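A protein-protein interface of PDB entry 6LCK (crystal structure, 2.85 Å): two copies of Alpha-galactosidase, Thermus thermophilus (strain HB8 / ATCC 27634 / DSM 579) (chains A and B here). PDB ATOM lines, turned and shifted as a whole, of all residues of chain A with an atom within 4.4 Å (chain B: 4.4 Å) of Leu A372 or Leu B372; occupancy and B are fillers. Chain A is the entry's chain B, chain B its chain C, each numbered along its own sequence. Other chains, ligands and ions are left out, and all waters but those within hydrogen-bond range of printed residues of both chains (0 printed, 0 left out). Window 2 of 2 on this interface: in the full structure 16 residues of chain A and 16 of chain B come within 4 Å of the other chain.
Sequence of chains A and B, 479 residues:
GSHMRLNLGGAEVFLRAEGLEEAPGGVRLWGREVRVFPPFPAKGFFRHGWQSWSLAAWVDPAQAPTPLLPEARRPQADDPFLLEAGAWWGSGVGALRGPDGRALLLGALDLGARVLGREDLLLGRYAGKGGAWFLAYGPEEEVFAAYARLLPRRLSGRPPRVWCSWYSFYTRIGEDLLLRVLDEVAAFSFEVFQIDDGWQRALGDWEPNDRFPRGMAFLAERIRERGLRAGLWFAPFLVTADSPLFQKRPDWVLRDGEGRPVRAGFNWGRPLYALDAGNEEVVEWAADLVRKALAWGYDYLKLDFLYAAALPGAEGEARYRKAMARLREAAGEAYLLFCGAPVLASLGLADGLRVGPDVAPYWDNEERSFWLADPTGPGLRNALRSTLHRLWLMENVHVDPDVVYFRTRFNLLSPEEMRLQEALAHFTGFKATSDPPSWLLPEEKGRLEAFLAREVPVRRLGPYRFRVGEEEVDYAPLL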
ATOM      1  N   PRO A  67       1.205  15.450  -2.055  1.00  0.00           N
ATOM      2  CA  PRO A  67       1.959  15.872  -3.243  1.00  0.00           C
ATOM      3  C   PRO A  67       1.961  14.794  -4.308  1.00  0.00           C
ATOM      4  O   PRO A  67       2.139  13.611  -4.024  1.00  0.00           O
ATOM      5  CB  PRO A  67       3.372  16.128  -2.706  1.00  0.00           C
ATOM      6  CG  PRO A  67       3.208  16.307  -1.239  1.00  0.00           C
ATOM      7  CD  PRO A  67       2.041  15.450  -0.842  1.00  0.00           C
ATOM      8  N   LEU A  68       1.747  15.217  -5.537  1.00  0.00           N
ATOM      9  CA  LEU A  68       1.746  14.335  -6.693  1.00  0.00           C
ATOM     10  C   LEU A  68       3.169  14.217  -7.229  1.00  0.00           C
ATOM     11  O   LEU A  68       3.879  15.222  -7.355  1.00  0.00           O
ATOM     12  CB  LEU A  68       0.795  14.889  -7.760  1.00  0.00           C
ATOM     13  CG  LEU A  68       0.500  14.131  -9.044  1.00  0.00           C
ATOM     14  CD1 LEU A  68      -0.951  14.350  -9.465  1.00  0.00           C
ATOM     15  CD2 LEU A  68       1.472  14.548 -10.133  1.00  0.00           C
ATOM     16  N   LEU A  69       3.592  12.993  -7.534  1.00  0.00           N
ATOM     17  CA  LEU A  69       4.957  12.753  -7.971  1.00  0.00           C
ATOM     18  C   LEU A  69       4.957  12.043  -9.314  1.00  0.00           C
ATOM     19  O   LEU A  69       3.965  11.399  -9.688  1.00  0.00           O
ATOM     20  CB  LEU A  69       5.733  11.915  -6.948  1.00  0.00           C
ATOM     21  CG  LEU A  69       5.865  12.539  -5.559  1.00  0.00           C
ATOM     22  CD1 LEU A  69       6.286  11.503  -4.544  1.00  0.00           C
ATOM     23  CD2 LEU A  69       6.848  13.663  -5.584  1.00  0.00           C
ATOM     24  N   GLU A 367       1.280   1.453  -8.340  1.00  0.00           N
ATOM     25  CA  GLU A 367       2.541   2.164  -8.208  1.00  0.00           C
ATOM     26  C   GLU A 367       2.383   3.642  -8.532  1.00  0.00           C
ATOM     27  O   GLU A 367       2.933   4.506  -7.838  1.00  0.00           O
ATOM     28  CB  GLU A 367       3.589   1.525  -9.100  1.00  0.00           C
ATOM     29  CG  GLU A 367       4.510   0.616  -8.306  1.00  0.00           C
ATOM     30  CD  GLU A 367       3.827  -0.666  -7.933  1.00  0.00           C
ATOM     31  OE1 GLU A 367       3.050  -1.153  -8.776  1.00  0.00           O
ATOM     32  OE2 GLU A 367       4.048  -1.175  -6.812  1.00  0.00           O
ATOM     33  N   ARG A 368       1.621   3.955  -9.568  1.00  0.00           N
ATOM     34  CA  ARG A 368       1.403   5.346  -9.924  1.00  0.00           C
ATOM     35  C   ARG A 368       0.297   5.999  -9.111  1.00  0.00           C
ATOM     36  O   ARG A 368       0.449   7.152  -8.691  1.00  0.00           O
ATOM     37  CB  ARG A 368       1.083   5.456 -11.403  1.00  0.00           C
ATOM     38  CG  ARG A 368       1.071   6.860 -11.860  1.00  0.00           C
ATOM     39  CD  ARG A 368       1.053   6.938 -13.355  1.00  0.00           C
ATOM     40  NE  ARG A 368       0.800   8.311 -13.746  1.00  0.00           N
ATOM     41  CZ  ARG A 368       0.858   8.768 -14.983  1.00  0.00           C
ATOM     42  NH1 ARG A 368       1.163   7.962 -15.994  1.00  0.00           N
ATOM     43  NH2 ARG A 368       0.596  10.043 -15.183  1.00  0.00           N
ATOM     44  N   PHE A 370      -0.961   5.129  -6.052  1.00  0.00           N
ATOM     45  CA  PHE A 370      -0.674   5.167  -4.618  1.00  0.00           C
ATOM     46  C   PHE A 370       0.745   5.650  -4.291  1.00  0.00           C
ATOM     47  O   PHE A 370       0.910   6.623  -3.549  1.00  0.00           O
ATOM     48  CB  PHE A 370      -0.934   3.785  -4.005  1.00  0.00           C
ATOM     49  CG  PHE A 370      -0.509   3.678  -2.573  1.00  0.00           C
ATOM     50  CD1 PHE A 370       0.741   3.149  -2.235  1.00  0.00           C
ATOM     51  CD2 PHE A 370      -1.347   4.124  -1.554  1.00  0.00           C
ATOM     52  CE1 PHE A 370       1.143   3.062  -0.901  1.00  0.00           C
ATOM     53  CE2 PHE A 370      -0.954   4.046  -0.226  1.00  0.00           C
ATOM     54  CZ  PHE A 370       0.295   3.510   0.106  1.00  0.00           C
ATOM     55  N   TRP A 371       1.789   4.976  -4.799  1.00  0.00           N
ATOM     56  CA  TRP A 371       3.137   5.331  -4.355  1.00  0.00           C
ATOM     57  C   TRP A 371       3.570   6.683  -4.910  1.00  0.00           C
ATOM     58  O   TRP A 371       4.331   7.413  -4.255  1.00  0.00           O
ATOM     59  CB  TRP A 371       4.145   4.230  -4.723  1.00  0.00           C
ATOM     60  CG  TRP A 371       3.990   2.957  -3.892  1.00  0.00           C
ATOM     61  CD1 TRP A 371       3.593   1.729  -4.341  1.00  0.00           C
ATOM     62  CD2 TRP A 371       4.223   2.808  -2.479  1.00  0.00           C
ATOM     63  NE1 TRP A 371       3.563   0.825  -3.304  1.00  0.00           N
ATOM     64  CE2 TRP A 371       3.947   1.456  -2.151  1.00  0.00           C
ATOM     65  CE3 TRP A 371       4.646   3.678  -1.464  1.00  0.00           C
ATOM     66  CZ2 TRP A 371       4.070   0.958  -0.846  1.00  0.00           C
ATOM     67  CZ3 TRP A 371       4.770   3.181  -0.171  1.00  0.00           C
ATOM     68  CH2 TRP A 371       4.475   1.833   0.127  1.00  0.00           C
ATOM     69  N   LEU A 372       3.071   7.061  -6.084  1.00  0.00           N
ATOM     70  CA  LEU A 372       3.367   8.367  -6.646  1.00  0.00           C
ATOM     71  C   LEU A 372       2.229   9.373  -6.470  1.00  0.00           C
ATOM     72  O   LEU A 372       2.368  10.522  -6.907  1.00  0.00           O
ATOM     73  CB  LEU A 372       3.720   8.220  -8.125  1.00  0.00           C
ATOM     74  CG  LEU A 372       4.968   7.392  -8.423  1.00  0.00           C
ATOM     75  CD1 LEU A 372       5.194   7.230  -9.934  1.00  0.00           C
ATOM     76  CD2 LEU A 372       6.144   8.043  -7.759  1.00  0.00           C
ATOM     77  N   ALA A 373       1.108   8.971  -5.855  1.00  0.00           N
ATOM     78  CA  ALA A 373       0.022   9.886  -5.483  1.00  0.00           C
ATOM     79  C   ALA A 373      -0.493  10.679  -6.693  1.00  0.00           C
ATOM     80  O   ALA A 373      -0.696  11.900  -6.641  1.00  0.00           O
ATOM     81  CB  ALA A 373       0.469  10.810  -4.352  1.00  0.00           C
ATOM     82  N   ASP A 374      -0.728   9.953  -7.787  1.00  0.00           N
ATOM     83  CA  ASP A 374      -1.044  10.508  -9.103  1.00  0.00           C
ATOM     84  C   ASP A 374      -2.298   9.825  -9.634  1.00  0.00           C
ATOM     85  O   ASP A 374      -2.215   8.812 -10.347  1.00  0.00           O
ATOM     86  CB  ASP A 374       0.138  10.310 -10.055  1.00  0.00           C
ATOM     87  CG  ASP A 374      -0.111  10.867 -11.450  1.00  0.00           C
ATOM     88  OD1 ASP A 374      -1.168  11.476 -11.687  1.00  0.00           O
ATOM     89  OD2 ASP A 374       0.779  10.688 -12.319  1.00  0.00           O
ATOM     90  N   PRO B  67      18.999   5.275  -5.860  1.00  0.00           N
ATOM     91  CA  PRO B  67      18.220   4.746  -4.732  1.00  0.00           C
ATOM     92  C   PRO B  67      16.962   4.050  -5.221  1.00  0.00           C
ATOM     93  O   PRO B  67      16.318   4.504  -6.167  1.00  0.00           O
ATOM     94  CB  PRO B  67      17.885   6.000  -3.913  1.00  0.00           C
ATOM     95  CG  PRO B  67      18.959   6.975  -4.257  1.00  0.00           C
ATOM     96  CD  PRO B  67      19.293   6.710  -5.705  1.00  0.00           C
ATOM     97  N   LEU B  68      16.627   2.931  -4.574  1.00  0.00           N
ATOM     98  CA  LEU B  68      15.384   2.208  -4.835  1.00  0.00           C
ATOM     99  C   LEU B  68      14.287   2.724  -3.909  1.00  0.00           C
ATOM    100  O   LEU B  68      14.512   2.922  -2.714  1.00  0.00           O
ATOM    101  CB  LEU B  68      15.577   0.698  -4.618  1.00  0.00           C
ATOM    102  CG  LEU B  68      14.497  -0.345  -4.979  1.00  0.00           C
ATOM    103  CD1 LEU B  68      15.139  -1.688  -5.280  1.00  0.00           C
ATOM    104  CD2 LEU B  68      13.388  -0.530  -3.936  1.00  0.00           C
ATOM    105  N   LEU B  69      13.095   2.911  -4.461  1.00  0.00           N
ATOM    106  CA  LEU B  69      11.948   3.441  -3.740  1.00  0.00           C
ATOM    107  C   LEU B  69      10.728   2.547  -3.922  1.00  0.00           C
ATOM    108  O   LEU B  69      10.614   1.824  -4.919  1.00  0.00           O
ATOM    109  CB  LEU B  69      11.603   4.861  -4.215  1.00  0.00           C
ATOM    110  CG  LEU B  69      12.718   5.901  -4.198  1.00  0.00           C
ATOM    111  CD1 LEU B  69      12.243   7.095  -4.974  1.00  0.00           C
ATOM    112  CD2 LEU B  69      13.114   6.270  -2.785  1.00  0.00           C
ATOM    113  N   GLU B 367       6.402   2.706 -14.052  1.00  0.00           N
ATOM    114  CA  GLU B 367       6.300   3.493 -12.831  1.00  0.00           C
ATOM    115  C   GLU B 367       7.137   2.896 -11.714  1.00  0.00           C
ATOM    116  O   GLU B 367       7.775   3.627 -10.952  1.00  0.00           O
ATOM    117  CB  GLU B 367       4.840   3.620 -12.408  1.00  0.00           C
ATOM    118  CG  GLU B 367       4.283   4.956 -12.822  1.00  0.00           C
ATOM    119  CD  GLU B 367       4.126   5.034 -14.316  1.00  0.00           C
ATOM    120  OE1 GLU B 367       3.722   4.007 -14.899  1.00  0.00           O
ATOM    121  OE2 GLU B 367       4.432   6.098 -14.896  1.00  0.00           O
ATOM    122  N   ARG B 368       7.161   1.573 -11.602  1.00  0.00           N
ATOM    123  CA  ARG B 368       8.020   0.955 -10.603  1.00  0.00           C
ATOM    124  C   ARG B 368       9.458   0.784 -11.105  1.00  0.00           C
ATOM    125  O   ARG B 368      10.406   1.036 -10.362  1.00  0.00           O
ATOM    126  CB  ARG B 368       7.412  -0.373 -10.188  1.00  0.00           C
ATOM    127  CG  ARG B 368       8.167  -1.109  -9.123  1.00  0.00           C
ATOM    128  CD  ARG B 368       7.337  -2.281  -8.649  1.00  0.00           C
ATOM    129  NE  ARG B 368       7.992  -2.960  -7.543  1.00  0.00           N
ATOM    130  CZ  ARG B 368       7.430  -3.894  -6.784  1.00  0.00           C
ATOM    131  NH1 ARG B 368       6.174  -4.302  -7.005  1.00  0.00           N
ATOM    132  NH2 ARG B 368       8.143  -4.408  -5.793  1.00  0.00           N
ATOM    133  N   PHE B 370      11.243   2.503 -13.577  1.00  0.00           N
ATOM    134  CA  PHE B 370      11.929   3.769 -13.820  1.00  0.00           C
ATOM    135  C   PHE B 370      11.745   4.752 -12.664  1.00  0.00           C
ATOM    136  O   PHE B 370      12.706   5.091 -11.972  1.00  0.00           O
ATOM    137  CB  PHE B 370      11.436   4.393 -15.136  1.00  0.00           C
ATOM    138  CG  PHE B 370      12.163   5.668 -15.518  1.00  0.00           C
ATOM    139  CD1 PHE B 370      13.520   5.649 -15.765  1.00  0.00           C
ATOM    140  CD2 PHE B 370      11.488   6.883 -15.621  1.00  0.00           C
ATOM    141  CE1 PHE B 370      14.202   6.803 -16.088  1.00  0.00           C
ATOM    142  CE2 PHE B 370      12.167   8.039 -15.959  1.00  0.00           C
ATOM    143  CZ  PHE B 370      13.534   7.993 -16.188  1.00  0.00           C
ATOM    144  N   TRP B 371      10.512   5.202 -12.432  1.00  0.00           N
ATOM    145  CA  TRP B 371      10.287   6.300 -11.494  1.00  0.00           C
ATOM    146  C   TRP B 371      10.538   5.897 -10.037  1.00  0.00           C
ATOM    147  O   TRP B 371      10.946   6.740  -9.232  1.00  0.00           O
ATOM    148  CB  TRP B 371       8.871   6.846 -11.665  1.00  0.00           C
ATOM    149  CG  TRP B 371       8.652   7.596 -12.948  1.00  0.00           C
ATOM    150  CD1 TRP B 371       7.873   7.211 -13.997  1.00  0.00           C
ATOM    151  CD2 TRP B 371       9.224   8.866 -13.320  1.00  0.00           C
ATOM    152  NE1 TRP B 371       7.913   8.159 -14.997  1.00  0.00           N
ATOM    153  CE2 TRP B 371       8.736   9.184 -14.607  1.00  0.00           C
ATOM    154  CE3 TRP B 371      10.103   9.759 -12.692  1.00  0.00           C
ATOM    155  CZ2 TRP B 371       9.092  10.358 -15.276  1.00  0.00           C
ATOM    156  CZ3 TRP B 371      10.451  10.919 -13.356  1.00  0.00           C
ATOM    157  CH2 TRP B 371       9.944  11.211 -14.634  1.00  0.00           C
ATOM    158  N   LEU B 372      10.290   4.640  -9.661  1.00  0.00           N
ATOM    159  CA  LEU B 372      10.669   4.166  -8.334  1.00  0.00           C
ATOM    160  C   LEU B 372      11.987   3.423  -8.353  1.00  0.00           C
ATOM    161  O   LEU B 372      12.414   2.939  -7.300  1.00  0.00           O
ATOM    162  CB  LEU B 372       9.591   3.265  -7.744  1.00  0.00           C
ATOM    163  CG  LEU B 372       8.252   3.951  -7.572  1.00  0.00           C
ATOM    164  CD1 LEU B 372       7.217   2.929  -7.220  1.00  0.00           C
ATOM    165  CD2 LEU B 372       8.357   5.028  -6.515  1.00  0.00           C
ATOM    166  N   ALA B 373      12.628   3.312  -9.525  1.00  0.00           N
ATOM    167  CA  ALA B 373      13.965   2.741  -9.646  1.00  0.00           C
ATOM    168  C   ALA B 373      14.043   1.379  -8.959  1.00  0.00           C
ATOM    169  O   ALA B 373      14.989   1.065  -8.226  1.00  0.00           O
ATOM    170  CB  ALA B 373      15.020   3.706  -9.099  1.00  0.00           C
ATOM    171  N   ASP B 374      13.022   0.556  -9.200  1.00  0.00           N
ATOM    172  CA  ASP B 374      12.873  -0.753  -8.562  1.00  0.00           C
ATOM    173  C   ASP B 374      12.808  -1.836  -9.636  1.00  0.00           C
ATOM    174  O   ASP B 374      11.717  -2.183 -10.115  1.00  0.00           O
ATOM    175  CB  ASP B 374      11.630  -0.778  -7.675  1.00  0.00           C
ATOM    176  CG  ASP B 374      11.429  -2.105  -6.999  1.00  0.00           C
ATOM    177  OD1 ASP B 374      12.327  -2.964  -7.120  1.00  0.00           O
ATOM    178  OD2 ASP B 374      10.369  -2.289  -6.350  1.00  0.00           O
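Among the printed residues, merely in contact across the chains: Glu A367 with Leu B372, Leu A372 with Glu B367 and Leu A372 with Leu B372.
Of the 10 printed residues of chain A, 3 touch a printed residue of chain B.
Printed residues of chain B that touch a printed residue of chain A: Glu B367, Arg B368 and Leu B372.
The guanidinium group (NH1) of Arg A368 is in salt-bridge range of the side-chain carboxylate (OE2) of Glu B367 (3.9 Å).
The guanidinium group (NH1) of Arg B368 lies within salt-bridge range of the side-chain carboxylate (OE2) of Glu A367 (3.8 Å).
OD2 of Asp A374 is in salt-bridge range of NE of Arg A368 (2.8 Å).
O of Arg B368 lies within hydrogen-bond range of N of Ala B373, 3.3 Å away.
The backbone carbonyl oxygen of Glu B367 is in hydrogen-bond range of the backbone NH of Leu B372 (3.0 Å).
The guanidinium group of Arg B368 lies within salt-bridge range of the side-chain carboxylate of Asp B374, 2.7 Å away.
O of Leu B372 lies within hydrogen-bond range of N of Leu B69 (2.9 Å).
The backbone NH (N) of Leu A372 is in hydrogen-bond range of the backbone carbonyl oxygen (O) of Glu A367 (3.1 Å).
Glu A367 touches Arg B368, and with the chains exchanged Arg A368 touches Glu B367.
Glu A367 touches Leu B372, and with the chains exchanged Leu A372 touches Glu B367.
Leu B372 touches its own counterpart, Leu A372.
Positions printed for both chains: 67, 68, 69, 367, 368, 370, 371, 372, 373 and 374.
Of the 5 pairs that touch across the chains among the printed residues, 5 have their exchanged pair printed and touching as well.
Printed residues of chain B within 4 Å of Glu A367: Arg B368 (3.6 Å) and Leu B372 (3.7 Å).
Of the printed residues of chain B, Arg A368 touches Glu B367 (3.5 Å).
Of the printed residues of chain A, Glu B367 touches Arg A368 and Leu A372.
Printed residues of chain A within 4 Å of Arg B368: Glu A367.
Phe B370 touches none of the printed residues of chain A.
Leu B372 touches two residues of chain A.
Asp B374 touches none of the printed residues of chain A.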
